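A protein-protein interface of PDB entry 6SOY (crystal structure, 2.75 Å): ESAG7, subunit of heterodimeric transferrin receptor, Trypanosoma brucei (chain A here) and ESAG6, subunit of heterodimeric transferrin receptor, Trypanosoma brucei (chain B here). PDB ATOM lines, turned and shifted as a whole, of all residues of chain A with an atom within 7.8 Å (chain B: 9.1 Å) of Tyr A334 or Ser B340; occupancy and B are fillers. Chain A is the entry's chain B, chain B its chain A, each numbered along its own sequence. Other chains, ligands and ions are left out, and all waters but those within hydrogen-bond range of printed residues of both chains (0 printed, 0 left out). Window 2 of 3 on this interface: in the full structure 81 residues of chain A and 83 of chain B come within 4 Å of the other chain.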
ATOM      1  N   MET A  73      35.064   3.139  11.835  1.00  0.00           N
ATOM      2  CA  MET A  73      33.632   3.227  11.537  1.00  0.00           C
ATOM      3  C   MET A  73      32.827   3.828  12.714  1.00  0.00           C
ATOM      4  O   MET A  73      31.672   3.444  12.928  1.00  0.00           O
ATOM      5  CB  MET A  73      33.077   1.863  11.094  1.00  0.00           C
ATOM      6  CG  MET A  73      33.749   1.305   9.862  1.00  0.00           C
ATOM      7  SD  MET A  73      33.815  -0.500   9.949  1.00  0.00           S
ATOM      8  CE  MET A  73      35.050  -0.864   8.622  1.00  0.00           C
ATOM      9  N   PHE A 328      32.122  -5.938  15.700  1.00  0.00           N
ATOM     10  CA  PHE A 328      32.647  -5.772  14.339  1.00  0.00           C
ATOM     11  C   PHE A 328      31.609  -6.202  13.310  1.00  0.00           C
ATOM     12  O   PHE A 328      31.299  -5.436  12.401  1.00  0.00           O
ATOM     13  CB  PHE A 328      33.975  -6.527  14.142  1.00  0.00           C
ATOM     14  CG  PHE A 328      34.551  -6.346  12.758  1.00  0.00           C
ATOM     15  CD1 PHE A 328      35.151  -5.147  12.388  1.00  0.00           C
ATOM     16  CD2 PHE A 328      34.461  -7.359  11.814  1.00  0.00           C
ATOM     17  CE1 PHE A 328      35.658  -4.969  11.100  1.00  0.00           C
ATOM     18  CE2 PHE A 328      34.975  -7.184  10.528  1.00  0.00           C
ATOM     19  CZ  PHE A 328      35.572  -5.993  10.180  1.00  0.00           C
ATOM     20  N   GLU A 329      31.051  -7.419  13.497  1.00  0.00           N
ATOM     21  CA  GLU A 329      29.984  -8.029  12.704  1.00  0.00           C
ATOM     22  C   GLU A 329      28.775  -7.082  12.622  1.00  0.00           C
ATOM     23  O   GLU A 329      28.117  -7.029  11.588  1.00  0.00           O
ATOM     24  CB  GLU A 329      29.542  -9.355  13.353  1.00  0.00           C
ATOM     25  CG  GLU A 329      30.554 -10.483  13.269  1.00  0.00           C
ATOM     26  CD  GLU A 329      30.044 -11.811  13.800  1.00  0.00           C
ATOM     27  OE1 GLU A 329      29.727 -11.897  15.010  1.00  0.00           O
ATOM     28  OE2 GLU A 329      29.968 -12.770  13.001  1.00  0.00           O
ATOM     29  N   VAL A 330      28.511  -6.320  13.704  1.00  0.00           N
ATOM     30  CA  VAL A 330      27.431  -5.335  13.803  1.00  0.00           C
ATOM     31  C   VAL A 330      27.634  -4.174  12.794  1.00  0.00           C
ATOM     32  O   VAL A 330      26.746  -3.970  11.959  1.00  0.00           O
ATOM     33  CB  VAL A 330      27.224  -4.867  15.277  1.00  0.00           C
ATOM     34  CG1 VAL A 330      26.487  -3.530  15.372  1.00  0.00           C
ATOM     35  CG2 VAL A 330      26.505  -5.938  16.091  1.00  0.00           C
ATOM     36  N   ILE A 331      28.788  -3.441  12.846  1.00  0.00           N
ATOM     37  CA  ILE A 331      29.057  -2.334  11.905  1.00  0.00           C
ATOM     38  C   ILE A 331      29.285  -2.888  10.485  1.00  0.00           C
ATOM     39  O   ILE A 331      28.902  -2.233   9.507  1.00  0.00           O
ATOM     40  CB  ILE A 331      30.159  -1.299  12.326  1.00  0.00           C
ATOM     41  CG1 ILE A 331      30.247  -1.088  13.863  1.00  0.00           C
ATOM     42  CG2 ILE A 331      29.933   0.047  11.605  1.00  0.00           C
ATOM     43  CD1 ILE A 331      31.543  -0.370  14.375  1.00  0.00           C
ATOM     44  N   GLN A 332      29.871  -4.111  10.388  1.00  0.00           N
ATOM     45  CA  GLN A 332      30.116  -4.818   9.129  1.00  0.00           C
ATOM     46  C   GLN A 332      28.795  -5.022   8.379  1.00  0.00           C
ATOM     47  O   GLN A 332      28.658  -4.542   7.251  1.00  0.00           O
ATOM     48  CB  GLN A 332      30.813  -6.171   9.373  1.00  0.00           C
ATOM     49  CG  GLN A 332      31.484  -6.735   8.124  1.00  0.00           C
ATOM     50  CD  GLN A 332      32.243  -8.032   8.315  1.00  0.00           C
ATOM     51  OE1 GLN A 332      31.784  -8.977   8.972  1.00  0.00           O
ATOM     52  NE2 GLN A 332      33.414  -8.116   7.703  1.00  0.00           N
ATOM     53  N   LYS A 333      27.811  -5.675   9.029  1.00  0.00           N
ATOM     54  CA  LYS A 333      26.493  -5.930   8.445  1.00  0.00           C
ATOM     55  C   LYS A 333      25.655  -4.646   8.266  1.00  0.00           C
ATOM     56  O   LYS A 333      24.731  -4.639   7.450  1.00  0.00           O
ATOM     57  CB  LYS A 333      25.736  -7.001   9.241  1.00  0.00           C
ATOM     58  CG  LYS A 333      26.394  -8.377   9.192  1.00  0.00           C
ATOM     59  CD  LYS A 333      25.917  -9.255  10.344  1.00  0.00           C
ATOM     60  CE  LYS A 333      27.007 -10.174  10.829  1.00  0.00           C
ATOM     61  NZ  LYS A 333      26.590 -10.939  12.036  1.00  0.00           N
ATOM     62  N   TYR A 334      25.991  -3.558   9.001  1.00  0.00           N
ATOM     63  CA  TYR A 334      25.309  -2.265   8.887  1.00  0.00           C
ATOM     64  C   TYR A 334      25.628  -1.615   7.524  1.00  0.00           C
ATOM     65  O   TYR A 334      24.704  -1.267   6.778  1.00  0.00           O
ATOM     66  CB  TYR A 334      25.705  -1.328  10.056  1.00  0.00           C
ATOM     67  CG  TYR A 334      25.162   0.087   9.948  1.00  0.00           C
ATOM     68  CD1 TYR A 334      23.826   0.365  10.223  1.00  0.00           C
ATOM     69  CD2 TYR A 334      25.993   1.150   9.604  1.00  0.00           C
ATOM     70  CE1 TYR A 334      23.323   1.661  10.126  1.00  0.00           C
ATOM     71  CE2 TYR A 334      25.498   2.450   9.496  1.00  0.00           C
ATOM     72  CZ  TYR A 334      24.162   2.703   9.765  1.00  0.00           C
ATOM     73  OH  TYR A 334      23.666   3.985   9.680  1.00  0.00           O
ATOM     74  N   LEU A 335      26.941  -1.484   7.209  1.00  0.00           N
ATOM     75  CA  LEU A 335      27.492  -0.857   6.004  1.00  0.00           C
ATOM     76  C   LEU A 335      27.220  -1.604   4.693  1.00  0.00           C
ATOM     77  O   LEU A 335      27.147  -0.956   3.646  1.00  0.00           O
ATOM     78  CB  LEU A 335      28.998  -0.611   6.172  1.00  0.00           C
ATOM     79  CG  LEU A 335      29.377   0.588   7.036  1.00  0.00           C
ATOM     80  CD1 LEU A 335      30.651   0.320   7.805  1.00  0.00           C
ATOM     81  CD2 LEU A 335      29.485   1.865   6.202  1.00  0.00           C
ATOM     82  N   TRP A 336      27.104  -2.950   4.740  1.00  0.00           N
ATOM     83  CA  TRP A 336      26.810  -3.790   3.575  1.00  0.00           C
ATOM     84  C   TRP A 336      25.427  -3.435   2.994  1.00  0.00           C
ATOM     85  O   TRP A 336      25.290  -3.309   1.776  1.00  0.00           O
ATOM     86  CB  TRP A 336      26.826  -5.276   3.971  1.00  0.00           C
ATOM     87  CG  TRP A 336      28.175  -5.902   4.190  1.00  0.00           C
ATOM     88  CD1 TRP A 336      29.392  -5.409   3.811  1.00  0.00           C
ATOM     89  CD2 TRP A 336      28.426  -7.198   4.758  1.00  0.00           C
ATOM     90  NE1 TRP A 336      30.388  -6.302   4.142  1.00  0.00           N
ATOM     91  CE2 TRP A 336      29.823  -7.409   4.721  1.00  0.00           C
ATOM     92  CE3 TRP A 336      27.604  -8.200   5.304  1.00  0.00           C
ATOM     93  CZ2 TRP A 336      30.412  -8.578   5.207  1.00  0.00           C
ATOM     94  CZ3 TRP A 336      28.192  -9.350   5.799  1.00  0.00           C
ATOM     95  CH2 TRP A 336      29.579  -9.528   5.753  1.00  0.00           C
ATOM     96  N   PHE A 337      24.414  -3.249   3.874  1.00  0.00           N
ATOM     97  CA  PHE A 337      23.037  -2.926   3.497  1.00  0.00           C
ATOM     98  C   PHE A 337      22.483  -1.771   4.325  1.00  0.00           C
ATOM     99  O   PHE A 337      22.716  -0.609   3.996  1.00  0.00           O
ATOM    100  CB  PHE A 337      22.116  -4.165   3.592  1.00  0.00           C
ATOM    101  CG  PHE A 337      22.685  -5.435   4.201  1.00  0.00           C
ATOM    102  CD1 PHE A 337      23.401  -6.341   3.423  1.00  0.00           C
ATOM    103  CD2 PHE A 337      22.429  -5.766   5.527  1.00  0.00           C
ATOM    104  CE1 PHE A 337      23.912  -7.521   3.981  1.00  0.00           C
ATOM    105  CE2 PHE A 337      22.928  -6.955   6.079  1.00  0.00           C
ATOM    106  CZ  PHE A 337      23.667  -7.823   5.302  1.00  0.00           C
ATOM    107  N   VAL B  72      27.567  -6.592  -2.805  1.00  0.00           N
ATOM    108  CA  VAL B  72      26.527  -6.349  -1.800  1.00  0.00           C
ATOM    109  C   VAL B  72      26.350  -4.834  -1.633  1.00  0.00           C
ATOM    110  O   VAL B  72      25.232  -4.340  -1.799  1.00  0.00           O
ATOM    111  CB  VAL B  72      26.802  -7.088  -0.462  1.00  0.00           C
ATOM    112  CG1 VAL B  72      25.803  -6.684   0.615  1.00  0.00           C
ATOM    113  CG2 VAL B  72      26.777  -8.604  -0.657  1.00  0.00           C
ATOM    114  N   MET B  73      27.458  -4.101  -1.382  1.00  0.00           N
ATOM    115  CA  MET B  73      27.473  -2.638  -1.231  1.00  0.00           C
ATOM    116  C   MET B  73      26.964  -1.917  -2.486  1.00  0.00           C
ATOM    117  O   MET B  73      26.195  -0.966  -2.371  1.00  0.00           O
ATOM    118  CB  MET B  73      28.881  -2.140  -0.873  1.00  0.00           C
ATOM    119  CG  MET B  73      29.366  -2.604   0.493  1.00  0.00           C
ATOM    120  SD  MET B  73      31.143  -2.317   0.750  1.00  0.00           S
ATOM    121  CE  MET B  73      31.106  -0.648   1.284  1.00  0.00           C
ATOM    122  N   ARG B  88      23.078 -12.267   3.676  1.00  0.00           N
ATOM    123  CA  ARG B  88      23.178 -11.963   5.101  1.00  0.00           C
ATOM    124  C   ARG B  88      23.878 -13.127   5.830  1.00  0.00           C
ATOM    125  O   ARG B  88      24.877 -12.893   6.508  1.00  0.00           O
ATOM    126  CB  ARG B  88      21.765 -11.731   5.668  1.00  0.00           C
ATOM    127  CG  ARG B  88      21.715 -11.064   7.037  1.00  0.00           C
ATOM    128  CD  ARG B  88      20.292 -11.001   7.584  1.00  0.00           C
ATOM    129  NE  ARG B  88      19.507  -9.905   7.004  1.00  0.00           N
ATOM    130  CZ  ARG B  88      19.251  -8.753   7.619  1.00  0.00           C
ATOM    131  NH1 ARG B  88      19.712  -8.526   8.843  1.00  0.00           N
ATOM    132  NH2 ARG B  88      18.526  -7.819   7.015  1.00  0.00           N
ATOM    133  N   THR B 333      33.840   1.756   0.604  1.00  0.00           N
ATOM    134  CA  THR B 333      33.687   1.727   2.073  1.00  0.00           C
ATOM    135  C   THR B 333      33.672   3.144   2.662  1.00  0.00           C
ATOM    136  O   THR B 333      32.928   3.407   3.607  1.00  0.00           O
ATOM    137  CB  THR B 333      34.726   0.797   2.747  1.00  0.00           C
ATOM    138  OG1 THR B 333      34.881  -0.405   1.990  1.00  0.00           O
ATOM    139  CG2 THR B 333      34.348   0.435   4.177  1.00  0.00           C
ATOM    140  N   ILE B 334      34.486   4.049   2.085  1.00  0.00           N
ATOM    141  CA  ILE B 334      34.591   5.453   2.488  1.00  0.00           C
ATOM    142  C   ILE B 334      33.336   6.239   2.046  1.00  0.00           C
ATOM    143  O   ILE B 334      32.899   7.147   2.759  1.00  0.00           O
ATOM    144  CB  ILE B 334      35.950   6.050   2.001  1.00  0.00           C
ATOM    145  CG1 ILE B 334      36.914   6.265   3.185  1.00  0.00           C
ATOM    146  CG2 ILE B 334      35.818   7.309   1.125  1.00  0.00           C
ATOM    147  CD1 ILE B 334      38.191   5.470   3.090  1.00  0.00           C
ATOM    148  N   ASN B 335      32.752   5.861   0.887  1.00  0.00           N
ATOM    149  CA  ASN B 335      31.532   6.462   0.352  1.00  0.00           C
ATOM    150  C   ASN B 335      30.315   5.985   1.157  1.00  0.00           C
ATOM    151  O   ASN B 335      29.481   6.813   1.521  1.00  0.00           O
ATOM    152  CB  ASN B 335      31.377   6.174  -1.152  1.00  0.00           C
ATOM    153  CG  ASN B 335      32.277   7.000  -2.056  1.00  0.00           C
ATOM    154  OD1 ASN B 335      32.526   8.194  -1.835  1.00  0.00           O
ATOM    155  ND2 ASN B 335      32.773   6.383  -3.119  1.00  0.00           N
ATOM    156  N   ARG B 336      30.246   4.666   1.480  1.00  0.00           N
ATOM    157  CA  ARG B 336      29.173   4.059   2.283  1.00  0.00           C
ATOM    158  C   ARG B 336      29.168   4.541   3.749  1.00  0.00           C
ATOM    159  O   ARG B 336      28.123   4.472   4.397  1.00  0.00           O
ATOM    160  CB  ARG B 336      29.209   2.521   2.212  1.00  0.00           C
ATOM    161  CG  ARG B 336      28.358   1.932   1.097  1.00  0.00           C
ATOM    162  CD  ARG B 336      26.980   1.554   1.581  1.00  0.00           C
ATOM    163  NE  ARG B 336      26.234   0.799   0.575  1.00  0.00           N
ATOM    164  CZ  ARG B 336      24.987   0.361   0.734  1.00  0.00           C
ATOM    165  NH1 ARG B 336      24.386  -0.316  -0.236  1.00  0.00           N
ATOM    166  NH2 ARG B 336      24.331   0.596   1.865  1.00  0.00           N
ATOM    167  N   LEU B 337      30.324   5.023   4.262  1.00  0.00           N
ATOM    168  CA  LEU B 337      30.479   5.563   5.620  1.00  0.00           C
ATOM    169  C   LEU B 337      30.029   7.029   5.691  1.00  0.00           C
ATOM    170  O   LEU B 337      29.525   7.470   6.728  1.00  0.00           O
ATOM    171  CB  LEU B 337      31.936   5.451   6.082  1.00  0.00           C
ATOM    172  CG  LEU B 337      32.226   4.374   7.112  1.00  0.00           C
ATOM    173  CD1 LEU B 337      33.636   3.856   6.960  1.00  0.00           C
ATOM    174  CD2 LEU B 337      31.978   4.883   8.529  1.00  0.00           C
ATOM    175  N   GLU B 338      30.234   7.779   4.588  1.00  0.00           N
ATOM    176  CA  GLU B 338      29.853   9.184   4.445  1.00  0.00           C
ATOM    177  C   GLU B 338      28.376   9.317   4.034  1.00  0.00           C
ATOM    178  O   GLU B 338      27.810  10.411   4.093  1.00  0.00           O
ATOM    179  CB  GLU B 338      30.790   9.885   3.447  1.00  0.00           C
ATOM    180  CG  GLU B 338      31.639  10.985   4.069  1.00  0.00           C
ATOM    181  CD  GLU B 338      32.460  10.612   5.290  1.00  0.00           C
ATOM    182  OE1 GLU B 338      33.334   9.719   5.181  1.00  0.00           O
ATOM    183  OE2 GLU B 338      32.229  11.220   6.361  1.00  0.00           O
ATOM    184  N   LEU B 339      27.765   8.182   3.634  1.00  0.00           N
ATOM    185  CA  LEU B 339      26.360   7.996   3.248  1.00  0.00           C
ATOM    186  C   LEU B 339      25.514   7.986   4.539  1.00  0.00           C
ATOM    187  O   LEU B 339      24.387   8.500   4.546  1.00  0.00           O
ATOM    188  CB  LEU B 339      26.231   6.633   2.526  1.00  0.00           C
ATOM    189  CG  LEU B 339      25.032   6.387   1.615  1.00  0.00           C
ATOM    190  CD1 LEU B 339      25.424   5.484   0.463  1.00  0.00           C
ATOM    191  CD2 LEU B 339      23.873   5.755   2.376  1.00  0.00           C
ATOM    192  N   SER B 340      26.064   7.357   5.614  1.00  0.00           N
ATOM    193  CA  SER B 340      25.466   7.264   6.948  1.00  0.00           C
ATOM    194  C   SER B 340      25.744   8.571   7.712  1.00  0.00           C
ATOM    195  O   SER B 340      24.821   9.127   8.314  1.00  0.00           O
ATOM    196  CB  SER B 340      26.015   6.056   7.703  1.00  0.00           C
ATOM    197  OG  SER B 340      27.431   6.086   7.791  1.00  0.00           O
ATOM    198  N   LYS B 341      26.998   9.093   7.623  1.00  0.00           N
ATOM    199  CA  LYS B 341      27.432  10.351   8.241  1.00  0.00           C
ATOM    200  C   LYS B 341      26.783  11.592   7.601  1.00  0.00           C
ATOM    201  O   LYS B 341      27.016  12.704   8.078  1.00  0.00           O
ATOM    202  CB  LYS B 341      28.962  10.471   8.221  1.00  0.00           C
ATOM    203  CG  LYS B 341      29.647   9.785   9.395  1.00  0.00           C
ATOM    204  CD  LYS B 341      31.144  10.093   9.422  1.00  0.00           C
ATOM    205  CE  LYS B 341      32.006   8.948   8.932  1.00  0.00           C
ATOM    206  NZ  LYS B 341      32.325   7.985  10.019  1.00  0.00           N
ATOM    207  N   ARG B 342      25.980  11.403   6.529  1.00  0.00           N
ATOM    208  CA  ARG B 342      25.246  12.452   5.809  1.00  0.00           C
ATOM    209  C   ARG B 342      23.995  11.886   5.154  1.00  0.00           C
ATOM    210  O   ARG B 342      23.358  10.995   5.710  1.00  0.00           O
ATOM    211  CB  ARG B 342      26.128  13.140   4.758  1.00  0.00           C
ATOM    212  CG  ARG B 342      26.326  14.618   5.026  1.00  0.00           C
ATOM    213  CD  ARG B 342      27.471  15.184   4.213  1.00  0.00           C
ATOM    214  NE  ARG B 342      27.914  16.474   4.743  1.00  0.00           N
ATOM    215  CZ  ARG B 342      28.807  17.264   4.155  1.00  0.00           C
ATOM    216  NH1 ARG B 342      29.362  16.909   3.002  1.00  0.00           N
ATOM    217  NH2 ARG B 342      29.147  18.420   4.711  1.00  0.00           N
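NH2 of Arg B336 lies within hydrogen-bond range of O of Phe A337, 2.9 Å away.
The side-chain hydroxyl (OG) of Ser B340 is in hydrogen-bond range of the backbone carbonyl oxygen (O) of Leu B337 (2.7 Å).
NH1 of Arg B336 sits at hydrogen-bond distance from O of Met B73 (2.9 Å).
Among the printed residues, merely in contact across the chains: Leu A335 with Arg B336 (3.3 Å), Trp A336 with Val B72 (3.6 Å), Tyr A334 with Ser B340 (3.7 Å), Phe A337 with Val B72 (3.7 Å), Trp A336 with Arg B336 (3.7 Å), Trp A336 with Met B73 (3.8 Å), Leu A335 with Leu B337 (3.8 Å) and Met A73 with Leu B337 (3.8 Å).
Tyr A334 touches one residue of chain B.
Ser B340 touches one residue of chain A.
Printed residues of chain B within 4 Å of Trp A336: Val B72, Met B73 and Arg B336.
Of the printed residues of chain B, Leu A335 touches Arg B336 (3.3 Å) and Leu B337 (3.8 Å).
Of the printed residues of chain A, Leu B337 touches Met A73 (3.8 Å) and Leu A335 (3.8 Å).
Printed residues of chain A within 4 Å of Met B73: Trp A336.
Of the printed residues of chain A, Val B72 touches Trp A336 and Phe A337.
Gln A332 touches none of the printed residues of chain B.
The nearest residue of chain A that does not touch Ser B340 is Leu A335 (5.0 Å).
Among the printed residues, no Asp or Glu carboxylate lies within 4 Å of a Lys or Arg side-chain nitrogen of the other chain.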
